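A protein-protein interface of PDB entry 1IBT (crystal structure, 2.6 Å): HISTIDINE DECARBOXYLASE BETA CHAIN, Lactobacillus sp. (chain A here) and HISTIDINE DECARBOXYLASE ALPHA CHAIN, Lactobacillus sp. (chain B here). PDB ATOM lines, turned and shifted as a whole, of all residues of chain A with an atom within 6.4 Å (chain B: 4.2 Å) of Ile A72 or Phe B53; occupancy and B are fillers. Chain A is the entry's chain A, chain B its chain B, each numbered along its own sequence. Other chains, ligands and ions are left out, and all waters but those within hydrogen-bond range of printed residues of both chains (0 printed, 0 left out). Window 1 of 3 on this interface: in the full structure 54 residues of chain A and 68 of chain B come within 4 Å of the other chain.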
ATOM      1  N   THR A  24     -13.067 -22.845 -27.927  1.00  0.00           N
ATOM      2  CA  THR A  24     -12.841 -21.998 -29.074  1.00  0.00           C
ATOM      3  C   THR A  24     -13.608 -22.725 -30.179  1.00  0.00           C
ATOM      4  O   THR A  24     -14.123 -23.838 -29.989  1.00  0.00           O
ATOM      5  CB  THR A  24     -11.352 -21.932 -29.425  1.00  0.00           C
ATOM      6  OG1 THR A  24     -10.773 -23.181 -29.107  1.00  0.00           O
ATOM      7  CG2 THR A  24     -10.626 -20.890 -28.642  1.00  0.00           C
ATOM      8  N   LYS A  42       1.102 -25.495 -33.823  1.00  0.00           N
ATOM      9  CA  LYS A  42       1.214 -26.813 -33.193  1.00  0.00           C
ATOM     10  C   LYS A  42       2.059 -27.708 -34.086  1.00  0.00           C
ATOM     11  O   LYS A  42       1.775 -27.809 -35.287  1.00  0.00           O
ATOM     12  CB  LYS A  42      -0.101 -27.539 -33.060  1.00  0.00           C
ATOM     13  CG  LYS A  42      -0.108 -28.672 -32.060  1.00  0.00           C
ATOM     14  CD  LYS A  42      -1.166 -29.667 -32.481  1.00  0.00           C
ATOM     15  CE  LYS A  42      -1.677 -30.528 -31.318  1.00  0.00           C
ATOM     16  NZ  LYS A  42      -0.762 -31.442 -30.669  1.00  0.00           N
ATOM     17  N   ALA A  65      -1.426 -37.614 -31.983  1.00  0.00           N
ATOM     18  CA  ALA A  65      -0.700 -36.354 -32.096  1.00  0.00           C
ATOM     19  C   ALA A  65      -1.642 -35.168 -31.825  1.00  0.00           C
ATOM     20  O   ALA A  65      -1.252 -34.185 -31.162  1.00  0.00           O
ATOM     21  CB  ALA A  65      -0.085 -36.224 -33.500  1.00  0.00           C
ATOM     22  N   GLU A  66      -2.908 -35.213 -32.284  1.00  0.00           N
ATOM     23  CA  GLU A  66      -3.945 -34.201 -31.994  1.00  0.00           C
ATOM     24  C   GLU A  66      -4.172 -34.013 -30.476  1.00  0.00           C
ATOM     25  O   GLU A  66      -4.351 -32.863 -30.050  1.00  0.00           O
ATOM     26  CB  GLU A  66      -5.317 -34.568 -32.580  1.00  0.00           C
ATOM     27  CG  GLU A  66      -5.426 -34.778 -34.069  1.00  0.00           C
ATOM     28  CD  GLU A  66      -6.880 -34.859 -34.552  1.00  0.00           C
ATOM     29  OE1 GLU A  66      -7.219 -34.111 -35.484  1.00  0.00           O
ATOM     30  OE2 GLU A  66      -7.670 -35.649 -33.997  1.00  0.00           O
ATOM     31  N   THR A  67      -4.181 -35.081 -29.646  1.00  0.00           N
ATOM     32  CA  THR A  67      -4.318 -35.034 -28.198  1.00  0.00           C
ATOM     33  C   THR A  67      -2.951 -35.032 -27.505  1.00  0.00           C
ATOM     34  O   THR A  67      -2.789 -35.284 -26.297  1.00  0.00           O
ATOM     35  CB  THR A  67      -5.175 -36.247 -27.725  1.00  0.00           C
ATOM     36  OG1 THR A  67      -4.436 -37.462 -27.885  1.00  0.00           O
ATOM     37  CG2 THR A  67      -6.448 -36.375 -28.557  1.00  0.00           C
ATOM     38  N   LYS A  68      -1.856 -34.838 -28.243  1.00  0.00           N
ATOM     39  CA  LYS A  68      -0.575 -34.720 -27.583  1.00  0.00           C
ATOM     40  C   LYS A  68      -0.358 -33.248 -27.432  1.00  0.00           C
ATOM     41  O   LYS A  68      -0.564 -32.519 -28.408  1.00  0.00           O
ATOM     42  CB  LYS A  68       0.588 -35.275 -28.398  1.00  0.00           C
ATOM     43  CG  LYS A  68       1.722 -35.635 -27.437  1.00  0.00           C
ATOM     44  CD  LYS A  68       1.566 -36.982 -26.657  1.00  0.00           C
ATOM     45  CE  LYS A  68       0.216 -37.427 -26.010  1.00  0.00           C
ATOM     46  NZ  LYS A  68      -0.761 -37.904 -27.012  1.00  0.00           N
ATOM     47  N   ASN A  69       0.027 -32.839 -26.222  1.00  0.00           N
ATOM     48  CA  ASN A  69       0.309 -31.449 -25.913  1.00  0.00           C
ATOM     49  C   ASN A  69      -0.890 -30.530 -26.089  1.00  0.00           C
ATOM     50  O   ASN A  69      -1.908 -30.842 -25.468  1.00  0.00           O
ATOM     51  CB  ASN A  69       1.457 -30.987 -26.771  1.00  0.00           C
ATOM     52  CG  ASN A  69       2.715 -31.031 -25.957  1.00  0.00           C
ATOM     53  OD1 ASN A  69       2.764 -31.045 -24.711  1.00  0.00           O
ATOM     54  ND2 ASN A  69       3.764 -31.091 -26.768  1.00  0.00           N
ATOM     55  N   ALA A  70      -0.818 -29.427 -26.868  1.00  0.00           N
ATOM     56  CA  ALA A  70      -1.927 -28.534 -27.141  1.00  0.00           C
ATOM     57  C   ALA A  70      -3.073 -29.347 -27.696  1.00  0.00           C
ATOM     58  O   ALA A  70      -2.971 -29.843 -28.811  1.00  0.00           O
ATOM     59  CB  ALA A  70      -1.499 -27.500 -28.166  1.00  0.00           C
ATOM     60  N   TYR A  71      -4.140 -29.526 -26.940  1.00  0.00           N
ATOM     61  CA  TYR A  71      -5.260 -30.354 -27.330  1.00  0.00           C
ATOM     62  C   TYR A  71      -6.180 -29.891 -28.456  1.00  0.00           C
ATOM     63  O   TYR A  71      -6.906 -28.916 -28.303  1.00  0.00           O
ATOM     64  CB  TYR A  71      -6.042 -30.589 -26.065  1.00  0.00           C
ATOM     65  CG  TYR A  71      -7.149 -31.595 -26.244  1.00  0.00           C
ATOM     66  CD1 TYR A  71      -6.865 -32.941 -26.073  1.00  0.00           C
ATOM     67  CD2 TYR A  71      -8.430 -31.175 -26.583  1.00  0.00           C
ATOM     68  CE1 TYR A  71      -7.869 -33.891 -26.240  1.00  0.00           C
ATOM     69  CE2 TYR A  71      -9.430 -32.127 -26.760  1.00  0.00           C
ATOM     70  CZ  TYR A  71      -9.142 -33.474 -26.584  1.00  0.00           C
ATOM     71  OH  TYR A  71     -10.144 -34.399 -26.739  1.00  0.00           O
ATOM     72  N   ILE A  72      -6.233 -30.548 -29.605  1.00  0.00           N
ATOM     73  CA  ILE A  72      -7.196 -30.199 -30.631  1.00  0.00           C
ATOM     74  C   ILE A  72      -7.900 -31.510 -30.920  1.00  0.00           C
ATOM     75  O   ILE A  72      -8.154 -31.858 -32.070  1.00  0.00           O
ATOM     76  CB  ILE A  72      -6.542 -29.690 -31.934  1.00  0.00           C
ATOM     77  CG1 ILE A  72      -5.567 -30.647 -32.555  1.00  0.00           C
ATOM     78  CG2 ILE A  72      -5.777 -28.465 -31.590  1.00  0.00           C
ATOM     79  CD1 ILE A  72      -5.562 -30.521 -34.082  1.00  0.00           C
ATOM     80  N   GLY A  73      -8.281 -32.288 -29.908  1.00  0.00           N
ATOM     81  CA  GLY A  73      -8.832 -33.596 -30.196  1.00  0.00           C
ATOM     82  C   GLY A  73     -10.251 -33.475 -30.689  1.00  0.00           C
ATOM     83  O   GLY A  73     -10.928 -32.567 -30.248  1.00  0.00           O
ATOM     84  N   GLN A  74     -10.787 -34.308 -31.560  1.00  0.00           N
ATOM     85  CA  GLN A  74     -12.197 -34.313 -31.934  1.00  0.00           C
ATOM     86  C   GLN A  74     -12.686 -33.106 -32.679  1.00  0.00           C
ATOM     87  O   GLN A  74     -13.813 -32.663 -32.539  1.00  0.00           O
ATOM     88  CB  GLN A  74     -13.095 -34.489 -30.722  1.00  0.00           C
ATOM     89  CG  GLN A  74     -12.820 -35.716 -29.902  1.00  0.00           C
ATOM     90  CD  GLN A  74     -13.786 -35.826 -28.750  1.00  0.00           C
ATOM     91  OE1 GLN A  74     -14.830 -36.454 -28.869  1.00  0.00           O
ATOM     92  NE2 GLN A  74     -13.549 -35.209 -27.611  1.00  0.00           N
ATOM     93  N   ILE A  75     -11.874 -32.645 -33.589  1.00  0.00           N
ATOM     94  CA  ILE A  75     -12.090 -31.433 -34.351  1.00  0.00           C
ATOM     95  C   ILE A  75     -12.383 -31.866 -35.766  1.00  0.00           C
ATOM     96  O   ILE A  75     -11.945 -32.947 -36.095  1.00  0.00           O
ATOM     97  CB  ILE A  75     -10.751 -30.663 -34.077  1.00  0.00           C
ATOM     98  CG1 ILE A  75     -11.180 -29.580 -33.163  1.00  0.00           C
ATOM     99  CG2 ILE A  75      -9.981 -30.123 -35.282  1.00  0.00           C
ATOM    100  CD1 ILE A  75     -11.767 -30.032 -31.817  1.00  0.00           C
ATOM    101  N   MET A  77     -11.095 -31.266 -38.892  1.00  0.00           N
ATOM    102  CA  MET A  77     -10.045 -30.533 -39.549  1.00  0.00           C
ATOM    103  C   MET A  77     -10.296 -30.327 -41.009  1.00  0.00           C
ATOM    104  O   MET A  77     -10.632 -31.247 -41.715  1.00  0.00           O
ATOM    105  CB  MET A  77      -8.786 -31.290 -39.299  1.00  0.00           C
ATOM    106  CG  MET A  77      -7.620 -30.924 -40.185  1.00  0.00           C
ATOM    107  SD  MET A  77      -6.089 -30.641 -39.277  1.00  0.00           S
ATOM    108  CE  MET A  77      -6.314 -31.523 -37.745  1.00  0.00           C
ATOM    109  N   LEU B  49       0.444 -21.662 -27.338  1.00  0.00           N
ATOM    110  CA  LEU B  49      -0.810 -22.316 -27.689  1.00  0.00           C
ATOM    111  C   LEU B  49      -1.173 -23.386 -26.683  1.00  0.00           C
ATOM    112  O   LEU B  49      -2.341 -23.720 -26.491  1.00  0.00           O
ATOM    113  CB  LEU B  49      -0.723 -22.965 -29.052  1.00  0.00           C
ATOM    114  CG  LEU B  49      -2.004 -23.544 -29.631  1.00  0.00           C
ATOM    115  CD1 LEU B  49      -2.753 -22.436 -30.282  1.00  0.00           C
ATOM    116  CD2 LEU B  49      -1.761 -24.482 -30.766  1.00  0.00           C
ATOM    117  N   VAL B  50      -0.202 -23.939 -25.977  1.00  0.00           N
ATOM    118  CA  VAL B  50      -0.489 -24.981 -25.004  1.00  0.00           C
ATOM    119  C   VAL B  50      -1.106 -24.304 -23.795  1.00  0.00           C
ATOM    120  O   VAL B  50      -2.059 -24.861 -23.233  1.00  0.00           O
ATOM    121  CB  VAL B  50       0.796 -25.745 -24.609  1.00  0.00           C
ATOM    122  CG1 VAL B  50       0.446 -26.973 -23.784  1.00  0.00           C
ATOM    123  CG2 VAL B  50       1.523 -26.161 -25.867  1.00  0.00           C
ATOM    124  N   GLU B  51      -0.630 -23.107 -23.413  1.00  0.00           N
ATOM    125  CA  GLU B  51      -1.254 -22.384 -22.314  1.00  0.00           C
ATOM    126  C   GLU B  51      -2.729 -22.094 -22.578  1.00  0.00           C
ATOM    127  O   GLU B  51      -3.588 -22.335 -21.716  1.00  0.00           O
ATOM    128  CB  GLU B  51      -0.576 -21.064 -22.059  1.00  0.00           C
ATOM    129  CG  GLU B  51       0.848 -21.131 -21.521  1.00  0.00           C
ATOM    130  CD  GLU B  51       1.037 -21.740 -20.143  1.00  0.00           C
ATOM    131  OE1 GLU B  51       0.110 -22.297 -19.542  1.00  0.00           O
ATOM    132  OE2 GLU B  51       2.162 -21.703 -19.641  1.00  0.00           O
ATOM    133  N   TYR B  52      -3.044 -21.621 -23.777  1.00  0.00           N
ATOM    134  CA  TYR B  52      -4.419 -21.377 -24.138  1.00  0.00           C
ATOM    135  C   TYR B  52      -5.257 -22.632 -24.348  1.00  0.00           C
ATOM    136  O   TYR B  52      -6.253 -22.745 -23.630  1.00  0.00           O
ATOM    137  CB  TYR B  52      -4.447 -20.551 -25.389  1.00  0.00           C
ATOM    138  CG  TYR B  52      -5.790 -19.898 -25.644  1.00  0.00           C
ATOM    139  CD1 TYR B  52      -6.322 -19.027 -24.701  1.00  0.00           C
ATOM    140  CD2 TYR B  52      -6.463 -20.143 -26.835  1.00  0.00           C
ATOM    141  CE1 TYR B  52      -7.527 -18.395 -24.958  1.00  0.00           C
ATOM    142  CE2 TYR B  52      -7.677 -19.508 -27.098  1.00  0.00           C
ATOM    143  CZ  TYR B  52      -8.193 -18.641 -26.151  1.00  0.00           C
ATOM    144  OH  TYR B  52      -9.396 -18.032 -26.380  1.00  0.00           O
ATOM    145  N   PHE B  53      -5.018 -23.601 -25.260  1.00  0.00           N
ATOM    146  CA  PHE B  53      -5.919 -24.738 -25.389  1.00  0.00           C
ATOM    147  C   PHE B  53      -5.840 -25.670 -24.231  1.00  0.00           C
ATOM    148  O   PHE B  53      -6.856 -26.225 -23.828  1.00  0.00           O
ATOM    149  CB  PHE B  53      -5.648 -25.598 -26.570  1.00  0.00           C
ATOM    150  CG  PHE B  53      -5.994 -25.022 -27.913  1.00  0.00           C
ATOM    151  CD1 PHE B  53      -5.676 -25.759 -29.039  1.00  0.00           C
ATOM    152  CD2 PHE B  53      -6.606 -23.770 -28.041  1.00  0.00           C
ATOM    153  CE1 PHE B  53      -5.971 -25.238 -30.296  1.00  0.00           C
ATOM    154  CE2 PHE B  53      -6.899 -23.256 -29.302  1.00  0.00           C
ATOM    155  CZ  PHE B  53      -6.579 -23.993 -30.438  1.00  0.00           C
ATOM    156  N   GLY B  54      -4.670 -25.818 -23.653  1.00  0.00           N
ATOM    157  CA  GLY B  54      -4.486 -26.746 -22.554  1.00  0.00           C
ATOM    158  C   GLY B  54      -4.168 -28.112 -23.119  1.00  0.00           C
ATOM    159  O   GLY B  54      -4.036 -28.265 -24.330  1.00  0.00           O
ATOM    160  N   ARG B  59      -7.547 -29.662 -19.816  1.00  0.00           N
ATOM    161  CA  ARG B  59      -8.289 -29.075 -20.925  1.00  0.00           C
ATOM    162  C   ARG B  59      -8.725 -27.629 -20.652  1.00  0.00           C
ATOM    163  O   ARG B  59      -9.435 -27.389 -19.675  1.00  0.00           O
ATOM    164  CB  ARG B  59      -9.494 -29.968 -21.191  1.00  0.00           C
ATOM    165  CG  ARG B  59      -9.283 -31.177 -22.085  1.00  0.00           C
ATOM    166  CD  ARG B  59     -10.565 -31.987 -21.867  1.00  0.00           C
ATOM    167  NE  ARG B  59     -11.058 -32.904 -22.914  1.00  0.00           N
ATOM    168  CZ  ARG B  59     -10.588 -34.151 -23.074  1.00  0.00           C
ATOM    169  NH1 ARG B  59      -9.599 -34.632 -22.300  1.00  0.00           N
ATOM    170  NH2 ARG B  59     -11.235 -34.962 -23.922  1.00  0.00           N
ATOM    171  N   ARG B  60      -8.291 -26.643 -21.448  1.00  0.00           N
ATOM    172  CA  ARG B  60      -8.660 -25.244 -21.254  1.00  0.00           C
ATOM    173  C   ARG B  60      -9.517 -24.718 -22.385  1.00  0.00           C
ATOM    174  O   ARG B  60     -10.654 -25.160 -22.503  1.00  0.00           O
ATOM    175  CB  ARG B  60      -7.431 -24.352 -21.150  1.00  0.00           C
ATOM    176  CG  ARG B  60      -6.674 -24.599 -19.892  1.00  0.00           C
ATOM    177  CD  ARG B  60      -5.403 -23.782 -19.836  1.00  0.00           C
ATOM    178  NE  ARG B  60      -4.666 -24.239 -18.669  1.00  0.00           N
ATOM    179  CZ  ARG B  60      -3.494 -23.733 -18.321  1.00  0.00           C
ATOM    180  NH1 ARG B  60      -2.927 -24.231 -17.232  1.00  0.00           N
ATOM    181  NH2 ARG B  60      -2.880 -22.801 -19.059  1.00  0.00           N
ATOM    182  N   HIS B  61      -9.117 -23.811 -23.273  1.00  0.00           N
ATOM    183  CA  HIS B  61     -10.042 -23.283 -24.263  1.00  0.00           C
ATOM    184  C   HIS B  61      -9.756 -23.908 -25.608  1.00  0.00           C
ATOM    185  O   HIS B  61      -9.402 -23.296 -26.610  1.00  0.00           O
ATOM    186  CB  HIS B  61      -9.910 -21.757 -24.270  1.00  0.00           C
ATOM    187  CG  HIS B  61     -10.323 -21.222 -22.903  1.00  0.00           C
ATOM    188  ND1 HIS B  61     -11.523 -21.248 -22.327  1.00  0.00           N
ATOM    189  CD2 HIS B  61      -9.458 -20.713 -21.964  1.00  0.00           C
ATOM    190  CE1 HIS B  61     -11.419 -20.805 -21.106  1.00  0.00           C
ATOM    191  NE2 HIS B  61     -10.166 -20.485 -20.893  1.00  0.00           N
ATOM    192  N   TYR B  62      -9.941 -25.213 -25.612  1.00  0.00           N
ATOM    193  CA  TYR B  62      -9.661 -26.030 -26.778  1.00  0.00           C
ATOM    194  C   TYR B  62     -10.802 -25.979 -27.758  1.00  0.00           C
ATOM    195  O   TYR B  62     -11.835 -25.430 -27.391  1.00  0.00           O
ATOM    196  CB  TYR B  62      -9.399 -27.443 -26.316  1.00  0.00           C
ATOM    197  CG  TYR B  62     -10.563 -28.128 -25.655  1.00  0.00           C
ATOM    198  CD1 TYR B  62     -10.707 -28.066 -24.272  1.00  0.00           C
ATOM    199  CD2 TYR B  62     -11.445 -28.858 -26.433  1.00  0.00           C
ATOM    200  CE1 TYR B  62     -11.743 -28.760 -23.661  1.00  0.00           C
ATOM    201  CE2 TYR B  62     -12.485 -29.543 -25.826  1.00  0.00           C
ATOM    202  CZ  TYR B  62     -12.624 -29.499 -24.441  1.00  0.00           C
ATOM    203  OH  TYR B  62     -13.605 -30.247 -23.822  1.00  0.00           O
ATOM    204  N   PRO B  63     -10.750 -26.460 -28.983  1.00  0.00           N
ATOM    205  CA  PRO B  63     -11.887 -26.367 -29.845  1.00  0.00           C
ATOM    206  C   PRO B  63     -13.030 -27.291 -29.449  1.00  0.00           C
ATOM    207  O   PRO B  63     -12.890 -28.364 -28.865  1.00  0.00           O
ATOM    208  CB  PRO B  63     -11.263 -26.608 -31.171  1.00  0.00           C
ATOM    209  CG  PRO B  63      -9.892 -26.027 -31.053  1.00  0.00           C
ATOM    210  CD  PRO B  63      -9.546 -26.683 -29.764  1.00  0.00           C
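Thr A24 touches Tyr B52 (CG2 to CE2, 3.6 Å). Phe B53 touches Thr A24 (CE2 to OG1, 3.9 Å). O of Asn A69 touches O of Gly B54, at 3.5 Å. CB of Ala A70 touches CD2 of Leu B49 (3.99 Å). Ala A70 touches Gly B54 (CA to O, 3.5 Å). CD1 of Phe B53 touches O of Tyr A71, 3.5 Å away. CB of Tyr B62 touches O of Tyr A71 (3.5 Å). Pro B63 touches Tyr A71 (CD to O, 3.8 Å). Ile A72 touches Phe B53 (CG2 to CE1, 3.5 Å). CB of Pro B63 touches CD1 of Ile A75, 3.5 Å away.
Printed residues of chain A that touch a printed residue of chain B: Thr A24, Asn A69, Ala A70, Tyr A71, Ile A72 and Ile A75. Among the printed residues, 15 pairs touch across the chains. Among the printed residues, no Asp or Glu carboxylate lies within 4 Å of a Lys or Arg side-chain nitrogen of the other chain.
Printed residues of chain B within 4 Å of Thr A24: Tyr B52 (3.6 Å), Phe B53 (3.9 Å), His B61 (2.9 Å), Tyr B62 (2.9 Å) and Pro B63 (3.3 Å). Of the printed residues of chain A, Tyr B62 touches Thr A24 (2.9 Å) and Tyr A71 (3.5 Å). Printed residues of chain A within 4 Å of His B61: Thr A24. Lys A42 touches none of the printed residues of chain B. Gly A73 touches none of the printed residues of chain B. The nearest printed residue of chain B that does not touch Ile A72 is Pro B63 (4.3 Å).
The backbone carbonyl oxygen (O) of His B61 is in hydrogen-bond range of the side-chain hydroxyl (OG1) of Thr A24, 2.9 Å away. O of Tyr B62 sits at hydrogen-bond distance from N of Thr A24. N of Tyr A71 is in hydrogen-bond range of O of Gly B54, 2.9 Å away. The guanidinium group of Arg B59 lies within hydrogen-bond range of the side-chain hydroxyl of Tyr A71. N of Pro B63 sits close to OG1 of Thr A24 (3.3 Å).
The side-chain amino group (NZ) of Lys A42 lies close to the backbone carbonyl oxygen (O) of Ala A70, 3.3 Å away. O of Glu A66 lies within hydrogen-bond range of N of Ile A72 (3.0 Å). The backbone carbonyl oxygen (O) of Tyr B52 is in hydrogen-bond range of the backbone NH (N) of His B61, 3.1 Å away. The backbone carbonyl oxygen of Phe B53 lies within hydrogen-bond range of the backbone NH of Arg B60, at 2.8 Å. The backbone carbonyl oxygen (O) of Phe B53 is in hydrogen-bond range of the backbone NH (N) of His B61.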
